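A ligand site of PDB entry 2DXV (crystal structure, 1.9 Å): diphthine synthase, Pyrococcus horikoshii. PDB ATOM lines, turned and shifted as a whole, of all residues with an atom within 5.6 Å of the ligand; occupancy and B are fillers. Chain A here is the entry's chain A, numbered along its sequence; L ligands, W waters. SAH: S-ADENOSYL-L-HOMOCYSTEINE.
An oxygen (O2') of the ligand sits at hydrogen-bond distance from the backbone NH of Leu 166 (2.9 Å). The backbone carbonyl oxygen of Leu 166 lies within hydrogen-bond range of an oxygen (O3') of the ligand (2.6 Å). An oxygen (O2') of the ligand lies within hydrogen-bond range of the backbone carbonyl oxygen (O) of His 234, 2.6 Å away. N of the ligand is in hydrogen-bond range of O of Val 90. The backbone NH of Ala 209 is in hydrogen-bond range of a nitrogen (N1) of the ligand, 3.0 Å away. The backbone carbonyl oxygen (O) of Ala 209 is in hydrogen-bond range of a nitrogen (N6) of the ligand (2.7 Å). An oxygen (O) of the ligand sits at hydrogen-bond distance from the side-chain hydroxyl (OG) of Ser 115, at 2.8 Å. The backbone NH (N) of Asp 87 lies within hydrogen-bond range of an oxygen (O) of the ligand. O of Asp 87 is in hydrogen-bond range of N of the ligand, at 2.8 Å. The backbone NH (N) of Ile 116 is in hydrogen-bond range of an oxygen (OXT) of the ligand, 3.0 Å away. O of Leu 10 sits at hydrogen-bond distance from N6 of the ligand. The backbone NH (N) of Arg 208 lies within hydrogen-bond range of a nitrogen (N1) of the ligand (3.5 Å).
OG of Ser 115 sits close to N of Tyr 117, at 3.2 Å. N of Leu 89 is in hydrogen-bond range of OD1 of Asp 87 (2.9 Å). N of Ile 235 is in hydrogen-bond range of O of Leu 206, at 3.0 Å. The backbone carbonyl oxygen (O) of Pro 233 lies within hydrogen-bond range of the backbone NH (N) of Arg 208 (3.0 Å). The side-chain hydroxyl of Thr 92 lies within hydrogen-bond range of the backbone carbonyl oxygen of Pro 88, at 2.7 Å.
O of Thr 36 sits close to SD of the ligand, at 3.7 Å. Ser 37 touches the ligand. O of Pro 85 touches N of the ligand, 3.9 Å away. Gly 86 touches the ligand (CA to O, 3.7 Å). Ala 91 touches the ligand. Thr 92 touches the ligand (CG2 to N, 3.8 Å). Phe 165 touches the ligand (CD1 to O4', 3.7 Å). Leu 206 touches the ligand. Pro 233 touches the ligand (O to C2, 3.4 Å). CD1 of Ile 235 touches O2' of the ligand, at 3.2 Å. Hydrophobic or aromatic side chains that line the ligand: Leu 10, Val 90, Ala 91, Ile 116, Phe 165, Leu 166, Ala 209, Pro 233 and Ile 235. Within 4 Å of the ligand: Leu 10, Thr 36, Ser 37, Pro 85, Gly 86, Asp 87, Val 90, Ala 91, Thr 92, Ser 115, Ile 116, Phe 165, Leu 166, Leu 206, Arg 208, Ala 209, Pro 233, His 234 and Ile 235. Along chain A the residues within 4 Å of the ligand span positions 10 to 235. The nearest printed residue that does not touch the ligand is Asp 167 (4.3 Å).
Water W2 lies within hydrogen-bond range of N of the ligand, OG1 of Thr 36 and O of Pro 85. Water W1 lies within hydrogen-bond range of an oxygen (O3') of the ligand and the backbone carbonyl oxygen of Asp 167.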
ATOM      1  N   LEU A  10      18.657 -21.297  -7.942  1.00  0.00           N
ATOM      2  CA  LEU A  10      18.555 -21.593  -6.515  1.00  0.00           C
ATOM      3  C   LEU A  10      17.783 -20.749  -5.520  1.00  0.00           C
ATOM      4  O   LEU A  10      17.078 -21.296  -4.671  1.00  0.00           O
ATOM      5  CB  LEU A  10      19.974 -21.736  -5.969  1.00  0.00           C
ATOM      6  CG  LEU A  10      20.943 -22.705  -6.645  1.00  0.00           C
ATOM      7  CD1 LEU A  10      22.355 -22.401  -6.208  1.00  0.00           C
ATOM      8  CD2 LEU A  10      20.560 -24.130  -6.318  1.00  0.00           C
ATOM      9  N   TYR A  11      17.916 -19.434  -5.589  1.00  0.00           N
ATOM     10  CA  TYR A  11      17.327 -18.575  -4.573  1.00  0.00           C
ATOM     11  C   TYR A  11      16.453 -17.396  -5.013  1.00  0.00           C
ATOM     12  O   TYR A  11      15.357 -17.214  -4.480  1.00  0.00           O
ATOM     13  CB  TYR A  11      18.484 -18.084  -3.691  1.00  0.00           C
ATOM     14  CG  TYR A  11      18.108 -17.246  -2.493  1.00  0.00           C
ATOM     15  CD1 TYR A  11      17.458 -17.817  -1.391  1.00  0.00           C
ATOM     16  CD2 TYR A  11      18.426 -15.896  -2.449  1.00  0.00           C
ATOM     17  CE1 TYR A  11      17.145 -17.043  -0.268  1.00  0.00           C
ATOM     18  CE2 TYR A  11      18.122 -15.113  -1.334  1.00  0.00           C
ATOM     19  CZ  TYR A  11      17.483 -15.698  -0.248  1.00  0.00           C
ATOM     20  OH  TYR A  11      17.190 -14.919   0.847  1.00  0.00           O
ATOM     21  N   THR A  36       8.158 -27.920  -7.232  1.00  0.00           N
ATOM     22  CA  THR A  36       9.284 -28.845  -7.138  1.00  0.00           C
ATOM     23  C   THR A  36      10.360 -28.331  -6.183  1.00  0.00           C
ATOM     24  O   THR A  36      11.160 -29.110  -5.672  1.00  0.00           O
ATOM     25  CB  THR A  36       9.935 -29.102  -8.510  1.00  0.00           C
ATOM     26  OG1 THR A  36      10.329 -27.859  -9.106  1.00  0.00           O
ATOM     27  CG2 THR A  36       8.967 -29.819  -9.437  1.00  0.00           C
ATOM     28  N   SER A  37      10.386 -27.029  -5.954  1.00  0.00           N
ATOM     29  CA  SER A  37      11.373 -26.470  -5.049  1.00  0.00           C
ATOM     30  C   SER A  37      10.942 -25.099  -4.542  1.00  0.00           C
ATOM     31  O   SER A  37       9.900 -24.577  -4.947  1.00  0.00           O
ATOM     32  CB  SER A  37      12.732 -26.354  -5.736  1.00  0.00           C
ATOM     33  OG  SER A  37      13.721 -25.934  -4.809  1.00  0.00           O
ATOM     34  N   LEU A  38      11.734 -24.522  -3.645  1.00  0.00           N
ATOM     35  CA  LEU A  38      11.434 -23.222  -3.073  1.00  0.00           C
ATOM     36  C   LEU A  38      12.535 -22.204  -3.324  1.00  0.00           C
ATOM     37  O   LEU A  38      13.694 -22.413  -2.967  1.00  0.00           O
ATOM     38  CB  LEU A  38      11.212 -23.362  -1.556  1.00  0.00           C
ATOM     39  CG  LEU A  38      10.974 -22.065  -0.778  1.00  0.00           C
ATOM     40  CD1 LEU A  38       9.663 -21.433  -1.226  1.00  0.00           C
ATOM     41  CD2 LEU A  38      10.952 -22.352   0.716  1.00  0.00           C
ATOM     42  N   PRO A  85      12.090 -23.859 -10.688  1.00  0.00           N
ATOM     43  CA  PRO A  85      13.147 -23.456  -9.765  1.00  0.00           C
ATOM     44  C   PRO A  85      14.371 -24.326 -10.097  1.00  0.00           C
ATOM     45  O   PRO A  85      14.228 -25.389 -10.703  1.00  0.00           O
ATOM     46  CB  PRO A  85      12.556 -23.822  -8.398  1.00  0.00           C
ATOM     47  CG  PRO A  85      11.079 -23.734  -8.620  1.00  0.00           C
ATOM     48  CD  PRO A  85      10.908 -24.368  -9.970  1.00  0.00           C
ATOM     49  N   GLY A  86      15.554 -23.859  -9.707  1.00  0.00           N
ATOM     50  CA  GLY A  86      16.781 -24.609  -9.960  1.00  0.00           C
ATOM     51  C   GLY A  86      16.947 -24.992 -11.416  1.00  0.00           C
ATOM     52  O   GLY A  86      16.716 -24.185 -12.306  1.00  0.00           O
ATOM     53  N   ASP A  87      17.377 -26.230 -11.649  1.00  0.00           N
ATOM     54  CA  ASP A  87      17.537 -26.756 -13.003  1.00  0.00           C
ATOM     55  C   ASP A  87      16.265 -27.554 -13.248  1.00  0.00           C
ATOM     56  O   ASP A  87      15.866 -28.387 -12.421  1.00  0.00           O
ATOM     57  CB  ASP A  87      18.775 -27.653 -13.091  1.00  0.00           C
ATOM     58  CG  ASP A  87      18.989 -28.195 -14.489  1.00  0.00           C
ATOM     59  OD1 ASP A  87      18.164 -29.016 -14.944  1.00  0.00           O
ATOM     60  OD2 ASP A  87      19.979 -27.783 -15.139  1.00  0.00           O
ATOM     61  N   PRO A  88      15.594 -27.317 -14.385  1.00  0.00           N
ATOM     62  CA  PRO A  88      14.348 -28.008 -14.712  1.00  0.00           C
ATOM     63  C   PRO A  88      14.328 -29.536 -14.752  1.00  0.00           C
ATOM     64  O   PRO A  88      13.263 -30.142 -14.594  1.00  0.00           O
ATOM     65  CB  PRO A  88      13.945 -27.379 -16.044  1.00  0.00           C
ATOM     66  CG  PRO A  88      15.265 -27.058 -16.671  1.00  0.00           C
ATOM     67  CD  PRO A  88      16.067 -26.505 -15.516  1.00  0.00           C
ATOM     68  N   LEU A  89      15.483 -30.164 -14.950  1.00  0.00           N
ATOM     69  CA  LEU A  89      15.534 -31.620 -15.056  1.00  0.00           C
ATOM     70  C   LEU A  89      16.249 -32.326 -13.915  1.00  0.00           C
ATOM     71  O   LEU A  89      16.580 -33.513 -14.032  1.00  0.00           O
ATOM     72  CB  LEU A  89      16.176 -32.022 -16.385  1.00  0.00           C
ATOM     73  CG  LEU A  89      15.553 -31.440 -17.643  1.00  0.00           C
ATOM     74  CD1 LEU A  89      16.296 -31.959 -18.874  1.00  0.00           C
ATOM     75  CD2 LEU A  89      14.078 -31.803 -17.726  1.00  0.00           C
ATOM     76  N   VAL A  90      16.506 -31.621 -12.827  1.00  0.00           N
ATOM     77  CA  VAL A  90      17.186 -32.239 -11.697  1.00  0.00           C
ATOM     78  C   VAL A  90      16.218 -32.511 -10.555  1.00  0.00           C
ATOM     79  O   VAL A  90      15.602 -31.587 -10.031  1.00  0.00           O
ATOM     80  CB  VAL A  90      18.312 -31.333 -11.159  1.00  0.00           C
ATOM     81  CG1 VAL A  90      18.927 -31.968  -9.907  1.00  0.00           C
ATOM     82  CG2 VAL A  90      19.383 -31.142 -12.226  1.00  0.00           C
ATOM     83  N   ALA A  91      16.094 -33.779 -10.184  1.00  0.00           N
ATOM     84  CA  ALA A  91      15.217 -34.158  -9.089  1.00  0.00           C
ATOM     85  C   ALA A  91      13.768 -33.759  -9.348  1.00  0.00           C
ATOM     86  O   ALA A  91      13.035 -33.400  -8.428  1.00  0.00           O
ATOM     87  CB  ALA A  91      15.716 -33.547  -7.782  1.00  0.00           C
ATOM     88  N   THR A  92      13.385 -33.790 -10.611  1.00  0.00           N
ATOM     89  CA  THR A  92      12.031 -33.569 -11.049  1.00  0.00           C
ATOM     90  C   THR A  92      11.721 -34.657 -12.054  1.00  0.00           C
ATOM     91  O   THR A  92      12.581 -35.448 -12.407  1.00  0.00           O
ATOM     92  CB  THR A  92      11.901 -32.189 -11.734  1.00  0.00           C
ATOM     93  OG1 THR A  92      12.450 -32.244 -13.052  1.00  0.00           O
ATOM     94  CG2 THR A  92      12.589 -31.075 -10.942  1.00  0.00           C
ATOM     95  N   PRO A 114      21.625 -22.873 -12.043  1.00  0.00           N
ATOM     96  CA  PRO A 114      22.288 -23.427 -10.856  1.00  0.00           C
ATOM     97  C   PRO A 114      21.350 -24.420 -10.155  1.00  0.00           C
ATOM     98  O   PRO A 114      20.177 -24.131  -9.956  1.00  0.00           O
ATOM     99  CB  PRO A 114      22.553 -22.198  -9.994  1.00  0.00           C
ATOM    100  CG  PRO A 114      22.676 -21.088 -10.989  1.00  0.00           C
ATOM    101  CD  PRO A 114      21.614 -21.389 -12.008  1.00  0.00           C
ATOM    102  N   SER A 115      21.887 -25.587  -9.812  1.00  0.00           N
ATOM    103  CA  SER A 115      21.123 -26.650  -9.148  1.00  0.00           C
ATOM    104  C   SER A 115      21.698 -26.965  -7.779  1.00  0.00           C
ATOM    105  O   SER A 115      22.903 -26.896  -7.573  1.00  0.00           O
ATOM    106  CB  SER A 115      21.156 -27.924 -10.004  1.00  0.00           C
ATOM    107  OG  SER A 115      20.518 -29.012  -9.344  1.00  0.00           O
ATOM    108  N   ILE A 116      20.834 -27.325  -6.832  1.00  0.00           N
ATOM    109  CA  ILE A 116      21.307 -27.650  -5.490  1.00  0.00           C
ATOM    110  C   ILE A 116      22.208 -28.892  -5.571  1.00  0.00           C
ATOM    111  O   ILE A 116      23.090 -29.079  -4.724  1.00  0.00           O
ATOM    112  CB  ILE A 116      20.131 -27.944  -4.536  1.00  0.00           C
ATOM    113  CG1 ILE A 116      20.653 -28.133  -3.101  1.00  0.00           C
ATOM    114  CG2 ILE A 116      19.381 -29.179  -4.984  1.00  0.00           C
ATOM    115  CD1 ILE A 116      21.358 -26.912  -2.520  1.00  0.00           C
ATOM    116  N   TYR A 117      21.990 -29.710  -6.582  1.00  0.00           N
ATOM    117  CA  TYR A 117      22.770 -30.928  -6.760  1.00  0.00           C
ATOM    118  C   TYR A 117      24.267 -30.635  -6.908  1.00  0.00           C
ATOM    119  O   TYR A 117      25.114 -31.404  -6.456  1.00  0.00           O
ATOM    120  CB  TYR A 117      22.231 -31.696  -7.976  1.00  0.00           C
ATOM    121  CG  TYR A 117      22.897 -33.025  -8.258  1.00  0.00           C
ATOM    122  CD1 TYR A 117      22.792 -34.096  -7.370  1.00  0.00           C
ATOM    123  CD2 TYR A 117      23.615 -33.217  -9.444  1.00  0.00           C
ATOM    124  CE1 TYR A 117      23.369 -35.328  -7.654  1.00  0.00           C
ATOM    125  CE2 TYR A 117      24.200 -34.440  -9.736  1.00  0.00           C
ATOM    126  CZ  TYR A 117      24.072 -35.502  -8.848  1.00  0.00           C
ATOM    127  OH  TYR A 117      24.659 -36.698  -9.159  1.00  0.00           O
ATOM    128  N   LEU A 164      20.835 -35.545   0.633  1.00  0.00           N
ATOM    129  CA  LEU A 164      19.443 -35.828   0.941  1.00  0.00           C
ATOM    130  C   LEU A 164      18.558 -34.641   0.630  1.00  0.00           C
ATOM    131  O   LEU A 164      18.599 -33.631   1.343  1.00  0.00           O
ATOM    132  CB  LEU A 164      19.286 -36.197   2.423  1.00  0.00           C
ATOM    133  CG  LEU A 164      20.082 -37.421   2.915  1.00  0.00           C
ATOM    134  CD1 LEU A 164      19.985 -37.502   4.431  1.00  0.00           C
ATOM    135  CD2 LEU A 164      19.538 -38.688   2.274  1.00  0.00           C
ATOM    136  N   PHE A 165      17.802 -34.747  -0.461  1.00  0.00           N
ATOM    137  CA  PHE A 165      16.858 -33.712  -0.841  1.00  0.00           C
ATOM    138  C   PHE A 165      15.791 -33.808   0.236  1.00  0.00           C
ATOM    139  O   PHE A 165      15.469 -34.906   0.684  1.00  0.00           O
ATOM    140  CB  PHE A 165      16.225 -34.052  -2.189  1.00  0.00           C
ATOM    141  CG  PHE A 165      17.178 -34.023  -3.357  1.00  0.00           C
ATOM    142  CD1 PHE A 165      17.508 -32.819  -3.974  1.00  0.00           C
ATOM    143  CD2 PHE A 165      17.744 -35.195  -3.833  1.00  0.00           C
ATOM    144  CE1 PHE A 165      18.381 -32.787  -5.063  1.00  0.00           C
ATOM    145  CE2 PHE A 165      18.625 -35.174  -4.926  1.00  0.00           C
ATOM    146  CZ  PHE A 165      18.933 -33.970  -5.540  1.00  0.00           C
ATOM    147  N   LEU A 166      15.244 -32.675   0.672  1.00  0.00           N
ATOM    148  CA  LEU A 166      14.207 -32.696   1.710  1.00  0.00           C
ATOM    149  C   LEU A 166      12.824 -32.460   1.115  1.00  0.00           C
ATOM    150  O   LEU A 166      12.669 -31.730   0.133  1.00  0.00           O
ATOM    151  CB  LEU A 166      14.534 -31.669   2.805  1.00  0.00           C
ATOM    152  CG  LEU A 166      15.913 -31.876   3.444  1.00  0.00           C
ATOM    153  CD1 LEU A 166      16.073 -30.941   4.626  1.00  0.00           C
ATOM    154  CD2 LEU A 166      16.082 -33.328   3.887  1.00  0.00           C
ATOM    155  N   ASP A 167      11.796 -33.068   1.717  1.00  0.00           N
ATOM    156  CA  ASP A 167      10.437 -32.964   1.214  1.00  0.00           C
ATOM    157  C   ASP A 167       9.852 -31.553   1.149  1.00  0.00           C
ATOM    158  O   ASP A 167      10.292 -30.645   1.864  1.00  0.00           O
ATOM    159  CB  ASP A 167       9.508 -33.856   2.043  1.00  0.00           C
ATOM    160  CG  ASP A 167       8.322 -34.371   1.249  1.00  0.00           C
ATOM    161  OD1 ASP A 167       8.131 -33.906   0.100  1.00  0.00           O
ATOM    162  OD2 ASP A 167       7.583 -35.240   1.760  1.00  0.00           O
ATOM    163  N   ILE A 168       8.869 -31.387   0.277  1.00  0.00           N
ATOM    164  CA  ILE A 168       8.201 -30.107   0.104  1.00  0.00           C
ATOM    165  C   ILE A 168       6.730 -30.299  -0.273  1.00  0.00           C
ATOM    166  O   ILE A 168       6.404 -31.122  -1.137  1.00  0.00           O
ATOM    167  CB  ILE A 168       8.886 -29.235  -0.988  1.00  0.00           C
ATOM    168  CG1 ILE A 168       8.066 -27.958  -1.230  1.00  0.00           C
ATOM    169  CG2 ILE A 168       9.038 -30.034  -2.279  1.00  0.00           C
ATOM    170  CD1 ILE A 168       8.655 -27.018  -2.274  1.00  0.00           C
ATOM    171  N   LEU A 206      23.007 -27.378   4.563  1.00  0.00           N
ATOM    172  CA  LEU A 206      23.156 -26.232   3.676  1.00  0.00           C
ATOM    173  C   LEU A 206      21.767 -25.649   3.539  1.00  0.00           C
ATOM    174  O   LEU A 206      20.843 -26.333   3.079  1.00  0.00           O
ATOM    175  CB  LEU A 206      23.694 -26.660   2.301  1.00  0.00           C
ATOM    176  CG  LEU A 206      23.765 -25.532   1.262  1.00  0.00           C
ATOM    177  CD1 LEU A 206      24.646 -24.392   1.757  1.00  0.00           C
ATOM    178  CD2 LEU A 206      24.319 -26.099  -0.052  1.00  0.00           C
ATOM    179  N   ALA A 207      21.614 -24.400   3.939  1.00  0.00           N
ATOM    180  CA  ALA A 207      20.316 -23.749   3.859  1.00  0.00           C
ATOM    181  C   ALA A 207      20.363 -22.517   2.969  1.00  0.00           C
ATOM    182  O   ALA A 207      21.267 -21.695   3.086  1.00  0.00           O
ATOM    183  CB  ALA A 207      19.836 -23.364   5.255  1.00  0.00           C
ATOM    184  N   ARG A 208      19.371 -22.403   2.092  1.00  0.00           N
ATOM    185  CA  ARG A 208      19.257 -21.275   1.191  1.00  0.00           C
ATOM    186  C   ARG A 208      20.485 -21.066   0.309  1.00  0.00           C
ATOM    187  O   ARG A 208      21.033 -19.968   0.226  1.00  0.00           O
ATOM    188  CB  ARG A 208      18.950 -19.997   1.995  1.00  0.00           C
ATOM    189  CG  ARG A 208      17.692 -20.106   2.871  1.00  0.00           C
ATOM    190  CD  ARG A 208      17.478 -18.830   3.688  1.00  0.00           C
ATOM    191  NE  ARG A 208      18.684 -18.491   4.428  1.00  0.00           N
ATOM    192  CZ  ARG A 208      19.168 -19.193   5.452  1.00  0.00           C
ATOM    193  NH1 ARG A 208      18.524 -20.281   5.882  1.00  0.00           N
ATOM    194  NH2 ARG A 208      20.304 -18.833   6.025  1.00  0.00           N
ATOM    195  N   ALA A 209      20.920 -22.146  -0.325  1.00  0.00           N
ATOM    196  CA  ALA A 209      22.052 -22.063  -1.245  1.00  0.00           C
ATOM    197  C   ALA A 209      21.617 -21.083  -2.324  1.00  0.00           C
ATOM    198  O   ALA A 209      20.432 -21.015  -2.664  1.00  0.00           O
ATOM    199  CB  ALA A 209      22.327 -23.431  -1.845  1.00  0.00           C
ATOM    200  N   GLY A 210      22.562 -20.333  -2.870  1.00  0.00           N
ATOM    201  CA  GLY A 210      22.206 -19.368  -3.900  1.00  0.00           C
ATOM    202  C   GLY A 210      22.184 -17.960  -3.320  1.00  0.00           C
ATOM    203  O   GLY A 210      22.520 -16.996  -4.003  1.00  0.00           O
ATOM    204  N   PRO A 233      14.633 -23.107   1.806  1.00  0.00           N
ATOM    205  CA  PRO A 233      14.823 -24.562   1.766  1.00  0.00           C
ATOM    206  C   PRO A 233      16.124 -25.027   2.413  1.00  0.00           C
ATOM    207  O   PRO A 233      17.096 -24.284   2.480  1.00  0.00           O
ATOM    208  CB  PRO A 233      14.771 -24.871   0.277  1.00  0.00           C
ATOM    209  CG  PRO A 233      15.474 -23.683  -0.315  1.00  0.00           C
ATOM    210  CD  PRO A 233      14.884 -22.515   0.474  1.00  0.00           C
ATOM    211  N   HIS A 234      16.118 -26.279   2.873  1.00  0.00           N
ATOM    212  CA  HIS A 234      17.277 -26.899   3.507  1.00  0.00           C
ATOM    213  C   HIS A 234      17.612 -28.188   2.785  1.00  0.00           C
ATOM    214  O   HIS A 234      16.749 -28.820   2.173  1.00  0.00           O
ATOM    215  CB  HIS A 234      16.991 -27.291   4.960  1.00  0.00           C
ATOM    216  CG  HIS A 234      16.773 -26.153   5.901  1.00  0.00           C
ATOM    217  ND1 HIS A 234      16.573 -26.337   7.254  1.00  0.00           N
ATOM    218  CD2 HIS A 234      16.736 -24.816   5.695  1.00  0.00           C
ATOM    219  CE1 HIS A 234      16.421 -25.162   7.832  1.00  0.00           C
ATOM    220  NE2 HIS A 234      16.508 -24.221   6.917  1.00  0.00           N
ATOM    221  N   ILE A 235      18.869 -28.583   2.877  1.00  0.00           N
ATOM    222  CA  ILE A 235      19.308 -29.843   2.312  1.00  0.00           C
ATOM    223  C   ILE A 235      20.199 -30.449   3.395  1.00  0.00           C
ATOM    224  O   ILE A 235      20.896 -29.723   4.108  1.00  0.00           O
ATOM    225  CB  ILE A 235      20.099 -29.639   0.999  1.00  0.00           C
ATOM    226  CG1 ILE A 235      20.022 -30.915   0.157  1.00  0.00           C
ATOM    227  CG2 ILE A 235      21.546 -29.296   1.279  1.00  0.00           C
ATOM    228  CD1 ILE A 235      18.653 -31.159  -0.387  1.00  0.00           C
HETATM  229  N   SAH L   1      15.416 -28.932  -9.710  1.00  0.00           N
HETATM  230  CA  SAH L   1      15.824 -28.422  -8.327  1.00  0.00           C
HETATM  231  CB  SAH L   1      15.648 -29.358  -7.181  1.00  0.00           C
HETATM  232  CG  SAH L   1      14.260 -29.923  -6.901  1.00  0.00           C
HETATM  233  SD  SAH L   1      14.372 -30.864  -5.330  1.00  0.00           S
HETATM  234  C   SAH L   1      17.344 -27.958  -8.447  1.00  0.00           C
HETATM  235  O   SAH L   1      17.923 -28.096  -9.542  1.00  0.00           O
HETATM  236  OXT SAH L   1      17.879 -27.459  -7.382  1.00  0.00           O
HETATM  237  C5' SAH L   1      13.926 -29.614  -4.203  1.00  0.00           C
HETATM  238  C4' SAH L   1      14.680 -29.826  -2.832  1.00  0.00           C
HETATM  239  O4' SAH L   1      16.094 -29.583  -3.047  1.00  0.00           O
HETATM  240  C3' SAH L   1      14.265 -28.900  -1.741  1.00  0.00           C
HETATM  241  O3' SAH L   1      13.153 -29.431  -1.041  1.00  0.00           O
HETATM  242  C2' SAH L   1      15.564 -28.784  -0.921  1.00  0.00           C
HETATM  243  O2' SAH L   1      15.727 -29.880  -0.023  1.00  0.00           O
HETATM  244  C1' SAH L   1      16.673 -28.694  -1.987  1.00  0.00           C
HETATM  245  N9  SAH L   1      16.911 -27.441  -2.456  1.00  0.00           N
HETATM  246  C8  SAH L   1      16.566 -26.737  -3.599  1.00  0.00           C
HETATM  247  N7  SAH L   1      17.021 -25.520  -3.675  1.00  0.00           N
HETATM  248  C5  SAH L   1      17.746 -25.347  -2.458  1.00  0.00           C
HETATM  249  C6  SAH L   1      18.491 -24.217  -1.930  1.00  0.00           C
HETATM  250  N6  SAH L   1      18.622 -23.045  -2.552  1.00  0.00           N
HETATM  251  N1  SAH L   1      19.070 -24.438  -0.698  1.00  0.00           N
HETATM  252  C2  SAH L   1      18.964 -25.616  -0.017  1.00  0.00           C
HETATM  253  N3  SAH L   1      18.275 -26.699  -0.483  1.00  0.00           N
HETATM  254  C4  SAH L   1      17.689 -26.506  -1.704  1.00  0.00           C
HETATM  255  O   HOH W   1      11.807 -28.165   1.072  1.00  0.00           O
HETATM  256  O   HOH W   2      13.016 -27.692  -9.506  1.00  0.00           O
